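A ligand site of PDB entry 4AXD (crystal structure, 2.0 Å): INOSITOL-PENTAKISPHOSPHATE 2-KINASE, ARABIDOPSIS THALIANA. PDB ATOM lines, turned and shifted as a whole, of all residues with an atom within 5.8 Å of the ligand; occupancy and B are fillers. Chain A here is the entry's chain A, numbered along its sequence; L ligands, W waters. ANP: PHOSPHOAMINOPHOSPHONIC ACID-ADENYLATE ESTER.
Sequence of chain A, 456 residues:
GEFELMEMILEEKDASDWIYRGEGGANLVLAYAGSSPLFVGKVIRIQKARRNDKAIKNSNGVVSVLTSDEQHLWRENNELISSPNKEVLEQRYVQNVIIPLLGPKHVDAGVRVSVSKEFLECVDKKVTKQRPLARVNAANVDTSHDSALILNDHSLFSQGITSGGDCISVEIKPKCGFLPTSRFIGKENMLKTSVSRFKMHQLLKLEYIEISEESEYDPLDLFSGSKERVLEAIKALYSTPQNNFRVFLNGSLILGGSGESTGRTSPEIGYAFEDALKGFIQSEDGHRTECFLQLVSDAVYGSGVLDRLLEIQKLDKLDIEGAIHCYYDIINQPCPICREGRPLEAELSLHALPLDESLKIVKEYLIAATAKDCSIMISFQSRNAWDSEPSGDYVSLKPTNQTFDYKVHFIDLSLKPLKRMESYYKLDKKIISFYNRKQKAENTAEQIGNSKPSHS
A nitrogen (N1) of the ligand is in hydrogen-bond range of the backbone NH (N) of His 154, 2.9 Å away. N of Ala 26 lies within hydrogen-bond range of O1B of the ligand (2.8 Å). O3' of the ligand sits at hydrogen-bond distance from OE2 of Glu 171 (2.6 Å). The backbone carbonyl oxygen (O) of Asn 152 is in hydrogen-bond range of a nitrogen (N6) of the ligand, 3.0 Å away. The backbone NH (N) of Asn 27 is in hydrogen-bond range of an oxygen (O1B) of the ligand (2.8 Å). An oxygen (O1B) of the ligand sits close to the backbone NH (N) of Gly 24 (3.4 Å). An oxygen (O2B) of the ligand is in hydrogen-bond range of the side-chain amide nitrogen (ND2) of Asn 27 (2.7 Å). An oxygen (O2B) of the ligand lies within salt-bridge range of the guanidinium group (NH2) of Arg 45 (2.6 Å). OD1 of Asp 412 is in hydrogen-bond range of N3B of the ligand, 3.0 Å away. N of Gly 25 lies within hydrogen-bond range of O1G of the ligand, at 2.7 Å.
Water W6 lies within hydrogen-bond range of an oxygen (O2B) of the ligand (2.6 Å), the guanidinium group of Arg 45 (3.3 Å), the side-chain carboxylate of Asp 412 (3.3 Å) and the side-chain hydroxyl of Ser 414 (3.4 Å). Water W4 lies within hydrogen-bond range of O1A of the ligand, OG of Ser 375 and OD2 of Asp 412. Water W5 lies within hydrogen-bond range of O3' of the ligand, NH2 of Arg 246 and O of Glu 23. Water W8 bridges the guanidinium group of Arg 45 and an oxygen (O2A) of the ligand. Water W2 bridges a nitrogen (N3) of the ligand and the guanidinium group (NH1) of Arg 21. Water W7 bridges O2' of the ligand and NH2 of Arg 246.
N of Asn 152 is in hydrogen-bond range of OD2 of Asp 108 (3.1 Å). The backbone carbonyl oxygen (O) of Val 29 is in hydrogen-bond range of the backbone NH (N) of Arg 21 (2.9 Å). OG of Ser 155 sits at hydrogen-bond distance from OD1 of Asp 153 (2.8 Å). N of Val 43 is in hydrogen-bond range of O of Leu 151, at 2.8 Å. The guanidinium group of Arg 21 is in salt-bridge range of the side-chain carboxylate of Asp 153 (2.9 Å). NH2 of Arg 45 is in salt-bridge range of OD1 of Asp 412, 3.7 Å away. The backbone NH (N) of Val 29 sits at hydrogen-bond distance from the backbone carbonyl oxygen (O) of Gly 22, 2.8 Å away. The guanidinium group (NE) of Arg 246 lies within salt-bridge range of the side-chain carboxylate (OE1) of Glu 171 (3.8 Å).
SD of Met 377 sits close to N3 of the ligand (3.7 Å). Arg 21 touches the ligand (NH1 to C2, 3.96 Å). Glu 23 touches the ligand (C to C5', 3.6 Å). CG2 of Val 29 touches O4' of the ligand, at 3.4 Å. CG2 of Val 43 touches C6 of the ligand, at 3.7 Å. Leu 151 touches the ligand (CB to N6, 3.9 Å). Asp 153 touches the ligand. N of Ser 155 touches C2 of the ligand, 3.9 Å away. Phe 248 touches the ligand. Ile 411 touches the ligand (CD1 to C2', 3.8 Å). Hydrophobic or aromatic side chains within 4 Å of the ligand: Ala 26, Val 29, Val 43, Leu 151, His 154, Phe 248, Met 377 and Ile 411. Within 4 Å of the ligand: Arg 21, Glu 23, Gly 24, Gly 25, Ala 26, Asn 27, Val 29, Val 43, Arg 45, Leu 151, Asn 152, Asp 153, His 154, Ser 155, Glu 171, Phe 248, Met 377, Ile 411 and Asp 412.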
ATOM      1  N   ARG A  21     -25.594  20.938   7.103  1.00  0.00           N
ATOM      2  CA  ARG A  21     -24.444  21.840   7.284  1.00  0.00           C
ATOM      3  C   ARG A  21     -23.427  21.675   6.163  1.00  0.00           C
ATOM      4  O   ARG A  21     -22.963  22.665   5.571  1.00  0.00           O
ATOM      5  CB  ARG A  21     -23.787  21.633   8.647  1.00  0.00           C
ATOM      6  CG  ARG A  21     -22.462  22.377   8.843  1.00  0.00           C
ATOM      7  CD  ARG A  21     -22.610  23.904   8.873  1.00  0.00           C
ATOM      8  NE  ARG A  21     -23.402  24.349  10.021  1.00  0.00           N
ATOM      9  CZ  ARG A  21     -22.948  24.437  11.262  1.00  0.00           C
ATOM     10  NH1 ARG A  21     -21.710  24.054  11.561  1.00  0.00           N
ATOM     11  NH2 ARG A  21     -23.749  24.843  12.230  1.00  0.00           N
ATOM     12  N   GLY A  22     -23.067  20.420   5.873  1.00  0.00           N
ATOM     13  CA  GLY A  22     -22.083  20.117   4.831  1.00  0.00           C
ATOM     14  C   GLY A  22     -21.846  18.641   4.667  1.00  0.00           C
ATOM     15  O   GLY A  22     -22.543  17.808   5.265  1.00  0.00           O
ATOM     16  N   GLU A  23     -20.845  18.304   3.876  1.00  0.00           N
ATOM     17  CA  GLU A  23     -20.545  16.932   3.565  1.00  0.00           C
ATOM     18  C   GLU A  23     -19.179  16.834   2.903  1.00  0.00           C
ATOM     19  O   GLU A  23     -18.686  17.816   2.341  1.00  0.00           O
ATOM     20  CB  GLU A  23     -21.618  16.343   2.630  1.00  0.00           C
ATOM     21  CG  GLU A  23     -21.609  16.914   1.221  1.00  0.00           C
ATOM     22  CD  GLU A  23     -22.787  16.418   0.406  1.00  0.00           C
ATOM     23  OE1 GLU A  23     -23.881  17.028   0.509  1.00  0.00           O
ATOM     24  OE2 GLU A  23     -22.612  15.440  -0.354  1.00  0.00           O
ATOM     25  N   GLY A  24     -18.592  15.648   2.977  1.00  0.00           N
ATOM     26  CA  GLY A  24     -17.437  15.309   2.165  1.00  0.00           C
ATOM     27  C   GLY A  24     -17.695  13.953   1.537  1.00  0.00           C
ATOM     28  O   GLY A  24     -18.843  13.516   1.454  1.00  0.00           O
ATOM     29  N   GLY A  25     -16.626  13.275   1.116  1.00  0.00           N
ATOM     30  CA  GLY A  25     -16.744  11.956   0.485  1.00  0.00           C
ATOM     31  C   GLY A  25     -17.320  10.809   1.313  1.00  0.00           C
ATOM     32  O   GLY A  25     -17.860   9.866   0.736  1.00  0.00           O
ATOM     33  N   ALA A  26     -17.187  10.859   2.626  1.00  0.00           N
ATOM     34  CA  ALA A  26     -17.639   9.751   3.489  1.00  0.00           C
ATOM     35  C   ALA A  26     -18.876  10.051   4.349  1.00  0.00           C
ATOM     36  O   ALA A  26     -19.609   9.122   4.706  1.00  0.00           O
ATOM     37  CB  ALA A  26     -16.513   9.248   4.382  1.00  0.00           C
ATOM     38  N   ASN A  27     -19.073  11.325   4.711  1.00  0.00           N
ATOM     39  CA  ASN A  27     -20.094  11.701   5.680  1.00  0.00           C
ATOM     40  C   ASN A  27     -20.972  12.901   5.307  1.00  0.00           C
ATOM     41  O   ASN A  27     -20.528  13.802   4.617  1.00  0.00           O
ATOM     42  CB  ASN A  27     -19.445  12.011   7.048  1.00  0.00           C
ATOM     43  CG  ASN A  27     -18.875  10.768   7.704  1.00  0.00           C
ATOM     44  OD1 ASN A  27     -19.602  10.000   8.314  1.00  0.00           O
ATOM     45  ND2 ASN A  27     -17.572  10.574   7.579  1.00  0.00           N
ATOM     46  N   LEU A  28     -22.209  12.872   5.796  1.00  0.00           N
ATOM     47  CA  LEU A  28     -23.083  14.027   5.857  1.00  0.00           C
ATOM     48  C   LEU A  28     -23.036  14.643   7.257  1.00  0.00           C
ATOM     49  O   LEU A  28     -23.053  13.918   8.258  1.00  0.00           O
ATOM     50  CB  LEU A  28     -24.539  13.619   5.539  1.00  0.00           C
ATOM     51  CG  LEU A  28     -25.147  13.673   4.124  1.00  0.00           C
ATOM     52  CD1 LEU A  28     -24.519  14.685   3.186  1.00  0.00           C
ATOM     53  CD2 LEU A  28     -25.332  12.339   3.433  1.00  0.00           C
ATOM     54  N   VAL A  29     -23.036  15.967   7.332  1.00  0.00           N
ATOM     55  CA  VAL A  29     -23.002  16.658   8.611  1.00  0.00           C
ATOM     56  C   VAL A  29     -24.223  17.579   8.709  1.00  0.00           C
ATOM     57  O   VAL A  29     -24.485  18.365   7.794  1.00  0.00           O
ATOM     58  CB  VAL A  29     -21.692  17.448   8.838  1.00  0.00           C
ATOM     59  CG1 VAL A  29     -21.683  18.106  10.221  1.00  0.00           C
ATOM     60  CG2 VAL A  29     -20.481  16.557   8.651  1.00  0.00           C
ATOM     61  N   VAL A  43     -23.271  18.978  16.295  1.00  0.00           N
ATOM     62  CA  VAL A  43     -23.567  18.520  14.939  1.00  0.00           C
ATOM     63  C   VAL A  43     -23.686  17.006  14.981  1.00  0.00           C
ATOM     64  O   VAL A  43     -23.253  16.381  15.950  1.00  0.00           O
ATOM     65  CB  VAL A  43     -22.496  18.930  13.893  1.00  0.00           C
ATOM     66  CG1 VAL A  43     -22.521  20.441  13.683  1.00  0.00           C
ATOM     67  CG2 VAL A  43     -21.107  18.437  14.284  1.00  0.00           C
ATOM     68  N   ARG A  45     -22.803  13.593  12.624  1.00  0.00           N
ATOM     69  CA  ARG A  45     -22.063  13.097  11.475  1.00  0.00           C
ATOM     70  C   ARG A  45     -22.615  11.732  11.114  1.00  0.00           C
ATOM     71  O   ARG A  45     -22.696  10.819  11.953  1.00  0.00           O
ATOM     72  CB  ARG A  45     -20.602  13.020  11.851  1.00  0.00           C
ATOM     73  CG  ARG A  45     -19.628  13.093  10.696  1.00  0.00           C
ATOM     74  CD  ARG A  45     -18.236  13.261  11.266  1.00  0.00           C
ATOM     75  NE  ARG A  45     -17.205  13.409  10.259  1.00  0.00           N
ATOM     76  CZ  ARG A  45     -16.317  12.465   9.968  1.00  0.00           C
ATOM     77  NH1 ARG A  45     -16.352  11.302  10.607  1.00  0.00           N
ATOM     78  NH2 ARG A  45     -15.390  12.692   9.057  1.00  0.00           N
ATOM     79  N   ASP A 108     -11.861  16.117  19.221  1.00  0.00           N
ATOM     80  CA  ASP A 108     -13.104  15.635  19.822  1.00  0.00           C
ATOM     81  C   ASP A 108     -13.491  14.351  19.091  1.00  0.00           C
ATOM     82  O   ASP A 108     -13.803  14.373  17.897  1.00  0.00           O
ATOM     83  CB  ASP A 108     -14.201  16.722  19.711  1.00  0.00           C
ATOM     84  CG  ASP A 108     -15.604  16.226  20.133  1.00  0.00           C
ATOM     85  OD1 ASP A 108     -15.750  15.241  20.895  1.00  0.00           O
ATOM     86  OD2 ASP A 108     -16.604  16.861  19.699  1.00  0.00           O
ATOM     87  N   LEU A 151     -20.968  15.373  17.683  1.00  0.00           N
ATOM     88  CA  LEU A 151     -19.750  16.129  17.937  1.00  0.00           C
ATOM     89  C   LEU A 151     -20.126  17.568  18.271  1.00  0.00           C
ATOM     90  O   LEU A 151     -21.158  18.072  17.810  1.00  0.00           O
ATOM     91  CB  LEU A 151     -18.885  16.133  16.675  1.00  0.00           C
ATOM     92  CG  LEU A 151     -18.445  14.747  16.189  1.00  0.00           C
ATOM     93  CD1 LEU A 151     -18.658  14.646  14.689  1.00  0.00           C
ATOM     94  CD2 LEU A 151     -17.004  14.481  16.575  1.00  0.00           C
ATOM     95  N   ASN A 152     -19.301  18.250  19.053  1.00  0.00           N
ATOM     96  CA  ASN A 152     -19.450  19.684  19.205  1.00  0.00           C
ATOM     97  C   ASN A 152     -19.295  20.372  17.863  1.00  0.00           C
ATOM     98  O   ASN A 152     -18.469  19.967  17.057  1.00  0.00           O
ATOM     99  CB  ASN A 152     -18.432  20.241  20.177  1.00  0.00           C
ATOM    100  CG  ASN A 152     -18.733  19.870  21.606  1.00  0.00           C
ATOM    101  OD1 ASN A 152     -17.859  19.380  22.323  1.00  0.00           O
ATOM    102  ND2 ASN A 152     -19.956  20.103  22.037  1.00  0.00           N
ATOM    103  N   ASP A 153     -20.071  21.425  17.656  1.00  0.00           N
ATOM    104  CA  ASP A 153     -20.035  22.215  16.445  1.00  0.00           C
ATOM    105  C   ASP A 153     -18.836  23.178  16.549  1.00  0.00           C
ATOM    106  O   ASP A 153     -18.876  24.179  17.274  1.00  0.00           O
ATOM    107  CB  ASP A 153     -21.357  22.979  16.315  1.00  0.00           C
ATOM    108  CG  ASP A 153     -21.451  23.788  15.038  1.00  0.00           C
ATOM    109  OD1 ASP A 153     -20.444  23.934  14.312  1.00  0.00           O
ATOM    110  OD2 ASP A 153     -22.566  24.283  14.776  1.00  0.00           O
ATOM    111  N   HIS A 154     -17.772  22.870  15.818  1.00  0.00           N
ATOM    112  CA  HIS A 154     -16.562  23.691  15.886  1.00  0.00           C
ATOM    113  C   HIS A 154     -16.617  24.926  15.035  1.00  0.00           C
ATOM    114  O   HIS A 154     -15.640  25.669  14.928  1.00  0.00           O
ATOM    115  CB  HIS A 154     -15.332  22.853  15.584  1.00  0.00           C
ATOM    116  CG  HIS A 154     -15.208  21.636  16.454  1.00  0.00           C
ATOM    117  ND1 HIS A 154     -15.284  21.694  17.805  1.00  0.00           N
ATOM    118  CD2 HIS A 154     -15.015  20.301  16.132  1.00  0.00           C
ATOM    119  CE1 HIS A 154     -15.167  20.460  18.307  1.00  0.00           C
ATOM    120  NE2 HIS A 154     -14.991  19.602  17.290  1.00  0.00           N
ATOM    121  N   SER A 155     -17.776  25.188  14.420  1.00  0.00           N
ATOM    122  CA  SER A 155     -18.002  26.478  13.801  1.00  0.00           C
ATOM    123  C   SER A 155     -18.395  27.488  14.875  1.00  0.00           C
ATOM    124  O   SER A 155     -18.418  28.693  14.627  1.00  0.00           O
ATOM    125  CB  SER A 155     -19.061  26.428  12.693  1.00  0.00           C
ATOM    126  OG  SER A 155     -20.360  26.468  13.246  1.00  0.00           O
ATOM    127  N   GLU A 171     -12.231  27.290   8.570  1.00  0.00           N
ATOM    128  CA  GLU A 171     -11.877  25.909   8.308  1.00  0.00           C
ATOM    129  C   GLU A 171     -10.792  25.811   7.211  1.00  0.00           C
ATOM    130  O   GLU A 171     -10.961  26.330   6.099  1.00  0.00           O
ATOM    131  CB  GLU A 171     -13.124  25.105   7.916  1.00  0.00           C
ATOM    132  CG  GLU A 171     -12.861  23.628   7.603  1.00  0.00           C
ATOM    133  CD  GLU A 171     -14.131  22.916   7.161  1.00  0.00           C
ATOM    134  OE1 GLU A 171     -15.225  23.440   7.422  1.00  0.00           O
ATOM    135  OE2 GLU A 171     -14.029  21.816   6.573  1.00  0.00           O
ATOM    136  N   LYS A 173      -8.184  23.204   5.066  1.00  0.00           N
ATOM    137  CA  LYS A 173      -7.676  21.877   4.656  1.00  0.00           C
ATOM    138  C   LYS A 173      -6.251  22.102   4.188  1.00  0.00           C
ATOM    139  O   LYS A 173      -6.022  22.517   3.044  1.00  0.00           O
ATOM    140  CB  LYS A 173      -8.518  21.307   3.517  1.00  0.00           C
ATOM    141  CG  LYS A 173      -8.188  19.856   3.170  1.00  0.00           C
ATOM    142  CD  LYS A 173      -8.926  19.422   1.910  1.00  0.00           C
ATOM    143  CE  LYS A 173     -10.398  19.140   2.205  1.00  0.00           C
ATOM    144  NZ  LYS A 173     -10.647  17.668   2.345  1.00  0.00           N
ATOM    145  N   ARG A 246     -12.611  27.932   4.044  1.00  0.00           N
ATOM    146  CA  ARG A 246     -13.981  28.385   4.205  1.00  0.00           C
ATOM    147  C   ARG A 246     -14.126  29.138   5.487  1.00  0.00           C
ATOM    148  O   ARG A 246     -13.416  28.846   6.394  1.00  0.00           O
ATOM    149  CB  ARG A 246     -14.974  27.257   4.314  1.00  0.00           C
ATOM    150  CG  ARG A 246     -14.770  26.135   3.504  1.00  0.00           C
ATOM    151  CD  ARG A 246     -14.803  24.887   4.260  1.00  0.00           C
ATOM    152  NE  ARG A 246     -15.641  23.947   3.639  1.00  0.00           N
ATOM    153  CZ  ARG A 246     -15.308  23.122   2.670  1.00  0.00           C
ATOM    154  NH1 ARG A 246     -14.097  23.042   2.157  1.00  0.00           N
ATOM    155  NH2 ARG A 246     -16.229  22.342   2.231  1.00  0.00           N
ATOM    156  N   PHE A 248     -17.151  30.601   8.357  1.00  0.00           N
ATOM    157  CA  PHE A 248     -18.524  30.542   8.845  1.00  0.00           C
ATOM    158  C   PHE A 248     -18.826  31.706   9.779  1.00  0.00           C
ATOM    159  O   PHE A 248     -17.992  32.081  10.596  1.00  0.00           O
ATOM    160  CB  PHE A 248     -18.779  29.234   9.611  1.00  0.00           C
ATOM    161  CG  PHE A 248     -18.594  27.998   8.771  1.00  0.00           C
ATOM    162  CD1 PHE A 248     -19.655  27.502   8.004  1.00  0.00           C
ATOM    163  CD2 PHE A 248     -17.395  27.301   8.793  1.00  0.00           C
ATOM    164  CE1 PHE A 248     -19.499  26.351   7.238  1.00  0.00           C
ATOM    165  CE2 PHE A 248     -17.223  26.154   8.026  1.00  0.00           C
ATOM    166  CZ  PHE A 248     -18.279  25.682   7.238  1.00  0.00           C
ATOM    167  N   ASP A 373      -4.756  14.618   5.168  1.00  0.00           N
ATOM    168  CA  ASP A 373      -6.078  14.828   4.579  1.00  0.00           C
ATOM    169  C   ASP A 373      -7.094  15.485   5.520  1.00  0.00           C
ATOM    170  O   ASP A 373      -8.235  15.691   5.160  1.00  0.00           O
ATOM    171  CB  ASP A 373      -6.643  13.488   4.067  1.00  0.00           C
ATOM    172  CG  ASP A 373      -5.906  12.973   2.832  1.00  0.00           C
ATOM    173  OD1 ASP A 373      -5.294  13.774   2.102  1.00  0.00           O
ATOM    174  OD2 ASP A 373      -5.916  11.748   2.591  1.00  0.00           O
ATOM    175  N   SER A 375      -8.729  18.400   8.342  1.00  0.00           N
ATOM    176  CA  SER A 375      -8.932  19.839   8.367  1.00  0.00           C
ATOM    177  C   SER A 375      -8.832  20.374   9.789  1.00  0.00           C
ATOM    178  O   SER A 375      -8.883  19.611  10.760  1.00  0.00           O
ATOM    179  CB  SER A 375     -10.264  20.218   7.703  1.00  0.00           C
ATOM    180  OG  SER A 375     -10.192  20.045   6.284  1.00  0.00           O
ATOM    181  N   MET A 377     -10.443  23.514  12.252  1.00  0.00           N
ATOM    182  CA  MET A 377     -11.477  24.542  12.427  1.00  0.00           C
ATOM    183  C   MET A 377     -11.012  25.398  13.574  1.00  0.00           C
ATOM    184  O   MET A 377     -10.761  24.887  14.671  1.00  0.00           O
ATOM    185  CB  MET A 377     -12.860  23.925  12.697  1.00  0.00           C
ATOM    186  CG  MET A 377     -13.421  23.109  11.530  1.00  0.00           C
ATOM    187  SD  MET A 377     -15.181  22.666  11.724  1.00  0.00           S
ATOM    188  CE  MET A 377     -15.926  24.232  11.334  1.00  0.00           C
ATOM    189  N   ILE A 411     -10.631  18.245  12.486  1.00  0.00           N
ATOM    190  CA  ILE A 411     -11.751  17.420  12.034  1.00  0.00           C
ATOM    191  C   ILE A 411     -11.324  16.510  10.901  1.00  0.00           C
ATOM    192  O   ILE A 411     -10.242  16.669  10.333  1.00  0.00           O
ATOM    193  CB  ILE A 411     -12.978  18.258  11.607  1.00  0.00           C
ATOM    194  CG1 ILE A 411     -12.639  19.179  10.426  1.00  0.00           C
ATOM    195  CG2 ILE A 411     -13.549  19.031  12.803  1.00  0.00           C
ATOM    196  CD1 ILE A 411     -13.867  19.650   9.649  1.00  0.00           C
ATOM    197  N   ASP A 412     -12.195  15.541  10.598  1.00  0.00           N
ATOM    198  CA  ASP A 412     -12.040  14.691   9.415  1.00  0.00           C
ATOM    199  C   ASP A 412     -10.774  13.853   9.564  1.00  0.00           C
ATOM    200  O   ASP A 412      -9.901  13.857   8.712  1.00  0.00           O
ATOM    201  CB  ASP A 412     -12.008  15.548   8.144  1.00  0.00           C
ATOM    202  CG  ASP A 412     -12.117  14.734   6.869  1.00  0.00           C
ATOM    203  OD1 ASP A 412     -12.419  13.529   6.952  1.00  0.00           O
ATOM    204  OD2 ASP A 412     -11.882  15.317   5.782  1.00  0.00           O
ATOM    205  N   SER A 414      -9.919  10.426   9.586  1.00  0.00           N
ATOM    206  CA  SER A 414     -10.447   9.108   9.313  1.00  0.00           C
ATOM    207  C   SER A 414      -9.353   8.078   9.064  1.00  0.00           C
ATOM    208  O   SER A 414      -8.268   8.403   8.568  1.00  0.00           O
ATOM    209  CB  SER A 414     -11.407   9.160   8.133  1.00  0.00           C
ATOM    210  OG  SER A 414     -10.838   9.918   7.094  1.00  0.00           O
ATOM    211  N   LYS A 416      -7.650   5.288   7.062  1.00  0.00           N
ATOM    212  CA  LYS A 416      -7.536   5.023   5.638  1.00  0.00           C
ATOM    213  C   LYS A 416      -7.426   3.509   5.390  1.00  0.00           C
ATOM    214  O   LYS A 416      -6.627   2.834   6.033  1.00  0.00           O
ATOM    215  CB  LYS A 416      -6.322   5.769   5.040  1.00  0.00           C
ATOM    216  CG  LYS A 416      -6.220   7.247   5.409  1.00  0.00           C
ATOM    217  CD  LYS A 416      -7.373   8.058   4.848  1.00  0.00           C
ATOM    218  CE  LYS A 416      -7.411   9.444   5.489  1.00  0.00           C
ATOM    219  NZ  LYS A 416      -8.557  10.263   4.973  1.00  0.00           N
HETATM  220  PG  ANP L   1     -13.757  13.699   3.392  1.00  0.00           P
HETATM  221  O1G ANP L   1     -14.419  14.392   2.116  1.00  0.00           O
HETATM  222  O2G ANP L   1     -12.210  14.129   3.568  1.00  0.00           O
HETATM  223  O3G ANP L   1     -13.904  12.229   3.241  1.00  0.00           O
HETATM  224  PB  ANP L   1     -16.066  13.593   5.376  1.00  0.00           P
HETATM  225  O1B ANP L   1     -16.919  13.040   4.308  1.00  0.00           O
HETATM  226  O2B ANP L   1     -15.988  12.505   6.560  1.00  0.00           O
HETATM  227  N3B ANP L   1     -14.507  14.134   4.885  1.00  0.00           N
HETATM  228  PA  ANP L   1     -16.053  15.946   6.935  1.00  0.00           P
HETATM  229  O1A ANP L   1     -14.953  16.638   6.165  1.00  0.00           O
HETATM  230  O2A ANP L   1     -15.770  15.267   8.244  1.00  0.00           O
HETATM  231  O3A ANP L   1     -16.797  14.906   5.956  1.00  0.00           O
HETATM  232  O5' ANP L   1     -17.260  16.968   7.173  1.00  0.00           O
HETATM  233  C5' ANP L   1     -17.820  17.695   6.093  1.00  0.00           C
HETATM  234  C4' ANP L   1     -17.960  19.166   6.491  1.00  0.00           C
HETATM  235  O4' ANP L   1     -18.797  19.270   7.633  1.00  0.00           O
HETATM  236  C3' ANP L   1     -16.650  19.810   6.899  1.00  0.00           C
HETATM  237  O3' ANP L   1     -15.941  20.331   5.762  1.00  0.00           O
HETATM  238  C2' ANP L   1     -17.064  20.860   7.919  1.00  0.00           C
HETATM  239  O2' ANP L   1     -17.417  22.093   7.322  1.00  0.00           O
HETATM  240  C1' ANP L   1     -18.326  20.270   8.528  1.00  0.00           C
HETATM  241  N9  ANP L   1     -17.987  19.649   9.832  1.00  0.00           N
HETATM  242  C8  ANP L   1     -17.473  18.416  10.039  1.00  0.00           C
HETATM  243  N7  ANP L   1     -17.301  18.191  11.356  1.00  0.00           N
HETATM  244  C5  ANP L   1     -17.693  19.298  12.010  1.00  0.00           C
HETATM  245  C6  ANP L   1     -17.781  19.724  13.422  1.00  0.00           C
HETATM  246  N6  ANP L   1     -17.379  18.920  14.436  1.00  0.00           N
HETATM  247  N1  ANP L   1     -18.271  20.960  13.665  1.00  0.00           N
HETATM  248  C2  ANP L   1     -18.658  21.782  12.675  1.00  0.00           C
HETATM  249  N3  ANP L   1     -18.615  21.464  11.371  1.00  0.00           N
HETATM  250  C4  ANP L   1     -18.141  20.251  10.995  1.00  0.00           C
HETATM  251  O   HOH W   1     -14.469  16.391   3.490  1.00  0.00           O
HETATM  252  O   HOH W   2     -19.278  23.736   9.826  1.00  0.00           O
HETATM  253  O   HOH W   3     -13.816  10.529   1.262  1.00  0.00           O
HETATM  254  O   HOH W   4     -12.903  18.330   6.410  1.00  0.00           O
HETATM  255  O   HOH W   5     -16.220  19.496   3.108  1.00  0.00           O
HETATM  256  O   HOH W   6     -14.110  10.649   6.784  1.00  0.00           O
HETATM  257  O   HOH W   7     -18.485  22.526   4.666  1.00  0.00           O
HETATM  258  O   HOH W   8     -15.899  15.694  11.015  1.00  0.00           O
